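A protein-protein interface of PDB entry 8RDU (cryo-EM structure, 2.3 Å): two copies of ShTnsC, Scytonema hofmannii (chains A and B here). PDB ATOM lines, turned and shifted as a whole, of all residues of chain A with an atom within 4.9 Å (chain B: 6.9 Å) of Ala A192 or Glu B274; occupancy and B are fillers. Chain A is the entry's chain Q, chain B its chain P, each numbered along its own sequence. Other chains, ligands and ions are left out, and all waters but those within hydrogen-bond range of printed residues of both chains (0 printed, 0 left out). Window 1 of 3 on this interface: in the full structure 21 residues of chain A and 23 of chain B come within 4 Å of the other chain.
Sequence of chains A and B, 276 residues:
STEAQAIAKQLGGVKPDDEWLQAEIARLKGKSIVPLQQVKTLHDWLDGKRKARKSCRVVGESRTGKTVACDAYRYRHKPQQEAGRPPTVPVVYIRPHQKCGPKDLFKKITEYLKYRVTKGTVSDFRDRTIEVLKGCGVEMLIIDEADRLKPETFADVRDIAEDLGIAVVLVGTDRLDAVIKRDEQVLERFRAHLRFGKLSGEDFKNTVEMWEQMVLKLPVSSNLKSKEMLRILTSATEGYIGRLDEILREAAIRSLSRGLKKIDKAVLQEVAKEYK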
ATOM      1  N   TRP A  45     -28.916  -8.141  14.761  1.00  0.00           N
ATOM      2  CA  TRP A  45     -29.189  -9.263  15.651  1.00  0.00           C
ATOM      3  C   TRP A  45     -30.471 -10.003  15.263  1.00  0.00           C
ATOM      4  O   TRP A  45     -30.475 -11.235  15.145  1.00  0.00           O
ATOM      5  CB  TRP A  45     -29.239  -8.736  17.087  1.00  0.00           C
ATOM      6  CG  TRP A  45     -29.189  -9.750  18.190  1.00  0.00           C
ATOM      7  CD1 TRP A  45     -28.096 -10.457  18.595  1.00  0.00           C
ATOM      8  CD2 TRP A  45     -30.239 -10.077  19.109  1.00  0.00           C
ATOM      9  NE1 TRP A  45     -28.418 -11.253  19.666  1.00  0.00           N
ATOM     10  CE2 TRP A  45     -29.725 -11.033  20.006  1.00  0.00           C
ATOM     11  CE3 TRP A  45     -31.571  -9.678  19.242  1.00  0.00           C
ATOM     12  CZ2 TRP A  45     -30.496 -11.592  21.022  1.00  0.00           C
ATOM     13  CZ3 TRP A  45     -32.331 -10.234  20.247  1.00  0.00           C
ATOM     14  CH2 TRP A  45     -31.792 -11.181  21.125  1.00  0.00           C
ATOM     15  N   LYS A  49     -30.892 -13.769  14.171  1.00  0.00           N
ATOM     16  CA  LYS A  49     -31.751 -14.671  14.929  1.00  0.00           C
ATOM     17  C   LYS A  49     -32.854 -15.272  14.063  1.00  0.00           C
ATOM     18  O   LYS A  49     -33.136 -16.472  14.152  1.00  0.00           O
ATOM     19  CB  LYS A  49     -32.359 -13.924  16.112  1.00  0.00           C
ATOM     20  CG  LYS A  49     -32.728 -14.816  17.263  1.00  0.00           C
ATOM     21  CD  LYS A  49     -31.483 -15.283  17.986  1.00  0.00           C
ATOM     22  CE  LYS A  49     -30.789 -14.107  18.658  1.00  0.00           C
ATOM     23  NZ  LYS A  49     -29.547 -14.509  19.371  1.00  0.00           N
ATOM     24  N   SER A  55     -35.605 -18.482  19.135  1.00  0.00           N
ATOM     25  CA  SER A  55     -36.352 -17.558  19.977  1.00  0.00           C
ATOM     26  C   SER A  55     -35.439 -16.809  20.937  1.00  0.00           C
ATOM     27  O   SER A  55     -34.364 -17.288  21.311  1.00  0.00           O
ATOM     28  CB  SER A  55     -37.422 -18.311  20.768  1.00  0.00           C
ATOM     29  OG  SER A  55     -38.596 -18.488  20.001  1.00  0.00           O
ATOM     30  N   CYS A  56     -35.880 -15.621  21.332  1.00  0.00           N
ATOM     31  CA  CYS A  56     -35.091 -14.738  22.183  1.00  0.00           C
ATOM     32  C   CYS A  56     -36.010 -13.660  22.744  1.00  0.00           C
ATOM     33  O   CYS A  56     -37.204 -13.612  22.441  1.00  0.00           O
ATOM     34  CB  CYS A  56     -33.923 -14.137  21.403  1.00  0.00           C
ATOM     35  SG  CYS A  56     -34.433 -12.996  20.103  1.00  0.00           S
ATOM     36  N   ARG A  57     -35.435 -12.787  23.568  1.00  0.00           N
ATOM     37  CA  ARG A  57     -36.123 -11.620  24.092  1.00  0.00           C
ATOM     38  C   ARG A  57     -35.275 -10.362  23.953  1.00  0.00           C
ATOM     39  O   ARG A  57     -34.045 -10.417  23.934  1.00  0.00           O
ATOM     40  CB  ARG A  57     -36.538 -11.853  25.554  1.00  0.00           C
ATOM     41  CG  ARG A  57     -35.394 -11.996  26.538  1.00  0.00           C
ATOM     42  CD  ARG A  57     -35.939 -12.376  27.910  1.00  0.00           C
ATOM     43  NE  ARG A  57     -35.004 -12.127  29.001  1.00  0.00           N
ATOM     44  CZ  ARG A  57     -33.848 -12.756  29.158  1.00  0.00           C
ATOM     45  NH1 ARG A  57     -33.495 -13.764  28.379  1.00  0.00           N
ATOM     46  NH2 ARG A  57     -33.040 -12.388  30.145  1.00  0.00           N
ATOM     47  N   PHE A 190     -36.435 -18.698  26.258  1.00  0.00           N
ATOM     48  CA  PHE A 190     -36.182 -17.297  25.949  1.00  0.00           C
ATOM     49  C   PHE A 190     -34.977 -16.749  26.710  1.00  0.00           C
ATOM     50  O   PHE A 190     -34.903 -15.552  27.003  1.00  0.00           O
ATOM     51  CB  PHE A 190     -37.439 -16.471  26.194  1.00  0.00           C
ATOM     52  CG  PHE A 190     -38.567 -16.840  25.281  1.00  0.00           C
ATOM     53  CD1 PHE A 190     -38.604 -16.354  23.984  1.00  0.00           C
ATOM     54  CD2 PHE A 190     -39.579 -17.681  25.704  1.00  0.00           C
ATOM     55  CE1 PHE A 190     -39.627 -16.694  23.131  1.00  0.00           C
ATOM     56  CE2 PHE A 190     -40.610 -18.025  24.854  1.00  0.00           C
ATOM     57  CZ  PHE A 190     -40.634 -17.529  23.565  1.00  0.00           C
ATOM     58  N   ARG A 191     -34.038 -17.631  27.048  1.00  0.00           N
ATOM     59  CA  ARG A 191     -32.831 -17.262  27.781  1.00  0.00           C
ATOM     60  C   ARG A 191     -31.968 -16.266  27.004  1.00  0.00           C
ATOM     61  O   ARG A 191     -31.383 -15.354  27.598  1.00  0.00           O
ATOM     62  CB  ARG A 191     -32.054 -18.539  28.096  1.00  0.00           C
ATOM     63  CG  ARG A 191     -30.735 -18.388  28.812  1.00  0.00           C
ATOM     64  CD  ARG A 191     -30.140 -19.773  28.991  1.00  0.00           C
ATOM     65  NE  ARG A 191     -30.089 -20.493  27.723  1.00  0.00           N
ATOM     66  CZ  ARG A 191     -29.113 -20.387  26.831  1.00  0.00           C
ATOM     67  NH1 ARG A 191     -27.957 -19.829  27.139  1.00  0.00           N
ATOM     68  NH2 ARG A 191     -29.274 -20.924  25.626  1.00  0.00           N
ATOM     69  N   ALA A 192     -31.866 -16.429  25.687  1.00  0.00           N
ATOM     70  CA  ALA A 192     -31.135 -15.475  24.857  1.00  0.00           C
ATOM     71  C   ALA A 192     -31.788 -14.099  24.915  1.00  0.00           C
ATOM     72  O   ALA A 192     -32.998 -13.961  24.714  1.00  0.00           O
ATOM     73  CB  ALA A 192     -31.069 -15.969  23.412  1.00  0.00           C
ATOM     74  N   HIS A 193     -30.981 -13.074  25.184  1.00  0.00           N
ATOM     75  CA  HIS A 193     -31.483 -11.712  25.285  1.00  0.00           C
ATOM     76  C   HIS A 193     -30.503 -10.733  24.657  1.00  0.00           C
ATOM     77  O   HIS A 193     -29.296 -10.983  24.596  1.00  0.00           O
ATOM     78  CB  HIS A 193     -31.716 -11.308  26.745  1.00  0.00           C
ATOM     79  CG  HIS A 193     -30.448 -11.135  27.525  1.00  0.00           C
ATOM     80  ND1 HIS A 193     -29.762  -9.942  27.576  1.00  0.00           N
ATOM     81  CD2 HIS A 193     -29.731 -12.012  28.265  1.00  0.00           C
ATOM     82  CE1 HIS A 193     -28.683 -10.087  28.323  1.00  0.00           C
ATOM     83  NE2 HIS A 193     -28.641 -11.335  28.753  1.00  0.00           N
ATOM     84  N   LEU A 194     -31.051  -9.606  24.208  1.00  0.00           N
ATOM     85  CA  LEU A 194     -30.305  -8.407  23.853  1.00  0.00           C
ATOM     86  C   LEU A 194     -30.595  -7.305  24.861  1.00  0.00           C
ATOM     87  O   LEU A 194     -31.759  -6.968  25.105  1.00  0.00           O
ATOM     88  CB  LEU A 194     -30.650  -7.929  22.441  1.00  0.00           C
ATOM     89  CG  LEU A 194     -29.971  -6.622  22.021  1.00  0.00           C
ATOM     90  CD1 LEU A 194     -28.478  -6.747  22.144  1.00  0.00           C
ATOM     91  CD2 LEU A 194     -30.342  -6.263  20.599  1.00  0.00           C
ATOM     92  N   GLU B 246     -28.213 -25.356  21.457  1.00  0.00           N
ATOM     93  CA  GLU B 246     -28.504 -24.009  20.976  1.00  0.00           C
ATOM     94  C   GLU B 246     -27.233 -23.220  20.693  1.00  0.00           C
ATOM     95  O   GLU B 246     -27.118 -22.577  19.644  1.00  0.00           O
ATOM     96  CB  GLU B 246     -29.369 -23.267  21.998  1.00  0.00           C
ATOM     97  CG  GLU B 246     -29.945 -21.940  21.508  1.00  0.00           C
ATOM     98  CD  GLU B 246     -28.959 -20.784  21.632  1.00  0.00           C
ATOM     99  OE1 GLU B 246     -28.503 -20.505  22.761  1.00  0.00           O
ATOM    100  OE2 GLU B 246     -28.637 -20.155  20.601  1.00  0.00           O
ATOM    101  N   GLU B 250     -25.848 -21.551  17.039  1.00  0.00           N
ATOM    102  CA  GLU B 250     -25.699 -20.104  16.918  1.00  0.00           C
ATOM    103  C   GLU B 250     -24.300 -19.734  16.436  1.00  0.00           C
ATOM    104  O   GLU B 250     -24.141 -18.949  15.495  1.00  0.00           O
ATOM    105  CB  GLU B 250     -25.993 -19.446  18.267  1.00  0.00           C
ATOM    106  CG  GLU B 250     -26.269 -17.950  18.233  1.00  0.00           C
ATOM    107  CD  GLU B 250     -27.684 -17.611  17.820  1.00  0.00           C
ATOM    108  OE1 GLU B 250     -28.412 -18.520  17.377  1.00  0.00           O
ATOM    109  OE2 GLU B 250     -28.076 -16.434  17.954  1.00  0.00           O
ATOM    110  N   ARG B 254     -23.091 -18.241  12.685  1.00  0.00           N
ATOM    111  CA  ARG B 254     -22.301 -17.014  12.647  1.00  0.00           C
ATOM    112  C   ARG B 254     -20.948 -17.224  11.973  1.00  0.00           C
ATOM    113  O   ARG B 254     -20.556 -16.445  11.099  1.00  0.00           O
ATOM    114  CB  ARG B 254     -22.137 -16.454  14.059  1.00  0.00           C
ATOM    115  CG  ARG B 254     -23.424 -15.856  14.589  1.00  0.00           C
ATOM    116  CD  ARG B 254     -23.277 -15.276  15.974  1.00  0.00           C
ATOM    117  NE  ARG B 254     -24.581 -14.951  16.533  1.00  0.00           N
ATOM    118  CZ  ARG B 254     -24.782 -14.107  17.535  1.00  0.00           C
ATOM    119  NH1 ARG B 254     -23.815 -13.321  17.982  1.00  0.00           N
ATOM    120  NH2 ARG B 254     -26.001 -13.994  18.054  1.00  0.00           N
ATOM    121  N   GLN B 269     -17.608 -17.273  22.635  1.00  0.00           N
ATOM    122  CA  GLN B 269     -17.815 -16.377  23.769  1.00  0.00           C
ATOM    123  C   GLN B 269     -18.833 -15.284  23.461  1.00  0.00           C
ATOM    124  O   GLN B 269     -19.590 -14.883  24.350  1.00  0.00           O
ATOM    125  CB  GLN B 269     -16.474 -15.769  24.193  1.00  0.00           C
ATOM    126  CG  GLN B 269     -15.972 -14.659  23.272  1.00  0.00           C
ATOM    127  CD  GLN B 269     -14.495 -14.349  23.434  1.00  0.00           C
ATOM    128  OE1 GLN B 269     -13.767 -15.054  24.134  1.00  0.00           O
ATOM    129  NE2 GLN B 269     -14.042 -13.293  22.769  1.00  0.00           N
ATOM    130  N   GLU B 270     -18.873 -14.795  22.219  1.00  0.00           N
ATOM    131  CA  GLU B 270     -19.886 -13.816  21.839  1.00  0.00           C
ATOM    132  C   GLU B 270     -21.292 -14.398  21.932  1.00  0.00           C
ATOM    133  O   GLU B 270     -22.212 -13.741  22.435  1.00  0.00           O
ATOM    134  CB  GLU B 270     -19.607 -13.292  20.429  1.00  0.00           C
ATOM    135  CG  GLU B 270     -20.622 -12.269  19.931  1.00  0.00           C
ATOM    136  CD  GLU B 270     -20.549 -12.044  18.429  1.00  0.00           C
ATOM    137  OE1 GLU B 270     -19.444 -11.781  17.916  1.00  0.00           O
ATOM    138  OE2 GLU B 270     -21.602 -12.113  17.763  1.00  0.00           O
ATOM    139  N   VAL B 271     -21.482 -15.626  21.443  1.00  0.00           N
ATOM    140  CA  VAL B 271     -22.760 -16.314  21.617  1.00  0.00           C
ATOM    141  C   VAL B 271     -23.048 -16.559  23.093  1.00  0.00           C
ATOM    142  O   VAL B 271     -24.119 -16.207  23.601  1.00  0.00           O
ATOM    143  CB  VAL B 271     -22.767 -17.632  20.819  1.00  0.00           C
ATOM    144  CG1 VAL B 271     -24.008 -18.441  21.149  1.00  0.00           C
ATOM    145  CG2 VAL B 271     -22.702 -17.350  19.330  1.00  0.00           C
ATOM    146  N   ALA B 272     -22.095 -17.166  23.803  1.00  0.00           N
ATOM    147  CA  ALA B 272     -22.259 -17.462  25.224  1.00  0.00           C
ATOM    148  C   ALA B 272     -22.487 -16.220  26.080  1.00  0.00           C
ATOM    149  O   ALA B 272     -22.933 -16.345  27.223  1.00  0.00           O
ATOM    150  CB  ALA B 272     -21.038 -18.222  25.741  1.00  0.00           C
ATOM    151  N   LYS B 273     -22.198 -15.031  25.555  1.00  0.00           N
ATOM    152  CA  LYS B 273     -22.440 -13.771  26.251  1.00  0.00           C
ATOM    153  C   LYS B 273     -23.873 -13.261  26.123  1.00  0.00           C
ATOM    154  O   LYS B 273     -24.246 -12.329  26.842  1.00  0.00           O
ATOM    155  CB  LYS B 273     -21.458 -12.709  25.740  1.00  0.00           C
ATOM    156  CG  LYS B 273     -21.416 -11.426  26.559  1.00  0.00           C
ATOM    157  CD  LYS B 273     -21.080 -11.722  28.011  1.00  0.00           C
ATOM    158  CE  LYS B 273     -20.835 -10.448  28.799  1.00  0.00           C
ATOM    159  NZ  LYS B 273     -22.092  -9.687  29.027  1.00  0.00           N
ATOM    160  N   GLU B 274     -24.695 -13.859  25.270  1.00  0.00           N
ATOM    161  CA  GLU B 274     -26.062 -13.393  25.075  1.00  0.00           C
ATOM    162  C   GLU B 274     -27.018 -13.786  26.209  1.00  0.00           C
ATOM    163  O   GLU B 274     -28.238 -13.701  26.024  1.00  0.00           O
ATOM    164  CB  GLU B 274     -26.593 -13.906  23.738  1.00  0.00           C
ATOM    165  CG  GLU B 274     -25.725 -13.500  22.559  1.00  0.00           C
ATOM    166  CD  GLU B 274     -26.467 -13.525  21.241  1.00  0.00           C
ATOM    167  OE1 GLU B 274     -27.647 -13.930  21.226  1.00  0.00           O
ATOM    168  OE2 GLU B 274     -25.866 -13.140  20.217  1.00  0.00           O
ATOM    169  N   TYR B 275     -26.502 -14.201  27.364  1.00  0.00           N
ATOM    170  CA  TYR B 275     -27.316 -14.780  28.432  1.00  0.00           C
ATOM    171  C   TYR B 275     -26.944 -14.212  29.801  1.00  0.00           C
ATOM    172  O   TYR B 275     -25.840 -14.418  30.304  1.00  0.00           O
ATOM    173  CB  TYR B 275     -27.172 -16.297  28.444  1.00  0.00           C
ATOM    174  CG  TYR B 275     -27.144 -16.898  27.065  1.00  0.00           C
ATOM    175  CD1 TYR B 275     -28.251 -16.825  26.238  1.00  0.00           C
ATOM    176  CD2 TYR B 275     -25.999 -17.501  26.574  1.00  0.00           C
ATOM    177  CE1 TYR B 275     -28.235 -17.372  24.978  1.00  0.00           C
ATOM    178  CE2 TYR B 275     -25.973 -18.040  25.310  1.00  0.00           C
ATOM    179  CZ  TYR B 275     -27.095 -17.975  24.515  1.00  0.00           C
ATOM    180  OH  TYR B 275     -27.080 -18.505  23.247  1.00  0.00           O
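The guanidinium group of Arg A191 lies within salt-bridge range of the side-chain carboxylate of Glu B246, at 3.0 Å.
The side-chain amino group (NZ) of Lys A49 lies within salt-bridge range of the side-chain carboxylate (OE2) of Glu B250 (2.8 Å).
The indole nitrogen of Trp A45 is in hydrogen-bond range of the side-chain carboxylate of Glu B274, at 3.2 Å.
OE1 of Glu B274 lies within salt-bridge range of NZ of Lys A49, at 2.7 Å.
The backbone carbonyl oxygen (O) of Glu B274 lies within hydrogen-bond range of the backbone NH (N) of His A193, 2.9 Å away.
OE1 of Glu B246 lies within hydrogen-bond range of OH of Tyr B275 (2.5 Å).
The side-chain carboxylate of Glu B250 lies within salt-bridge range of the guanidinium group of Arg B254 (3.2 Å).
The guanidinium group (NH1) of Arg B254 lies within salt-bridge range of the side-chain carboxylate (OE2) of Glu B270.
The guanidinium group of Arg B254 is in salt-bridge range of the side-chain carboxylate of Glu B274 (3.0 Å).
The guanidinium group of Arg A57 lies within hydrogen-bond range of the backbone carbonyl oxygen of Arg A191 (2.8 Å).
The backbone NH (N) of Arg A57 sits at hydrogen-bond distance from the backbone carbonyl oxygen (O) of Ala A192 (2.9 Å).
Among the printed residues, pairs that only touch across the chains: Arg A191 with Tyr B275 (3.0 Å), Ala A192 with Tyr B275 (3.5 Å), His A193 with Tyr B275 (3.5 Å), Ala A192 with Glu B274 (3.6 Å), Lys A49 with Arg B254 (3.8 Å), Arg A191 with Glu B274 (3.9 Å) and Trp A45 with Arg B254 (3.99 Å).
Of the printed residues of chain B, Lys A49 touches Glu B250 (2.8 Å), Arg B254 (3.8 Å) and Glu B274 (2.7 Å).
Arg A57 touches none of the printed residues of chain B.
Ala A192 touches just these residues of chain B: Glu B274 and Tyr B275.
Of the printed residues of chain A, Glu B250 touches Lys A49.
Of the printed residues of chain A, Arg B254 touches Trp A45 and Lys A49.
Of chain A, only Trp A45 (3.2 Å), Lys A49 (2.7 Å), Arg A191 (3.9 Å), Ala A192 (3.6 Å) and His A193 (2.9 Å) come within 4 Å of Glu B274.
Of the printed residues of chain A, Tyr B275 touches Arg A191 (3.0 Å), Ala A192 (3.5 Å) and His A193 (3.5 Å).
The nearest residue of chain B that does not touch Ala A192 is Glu B246 (5.3 Å).
The nearest printed residue of chain B that does not touch Lys A49 is Glu B246 (5.8 Å).
Printed residues of chain A that touch a printed residue of chain B: Trp A45, Lys A49, Arg A191, Ala A192 and His A193.
Hydrophobic or aromatic side chains of chain A that line the printed part of chain B: Trp A45, Ala A192 and His A193.
No position is printed for both chains.
Of the 12 pairs that touch across the chains among the printed residues, none has its exchanged pair printed and touching as well.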
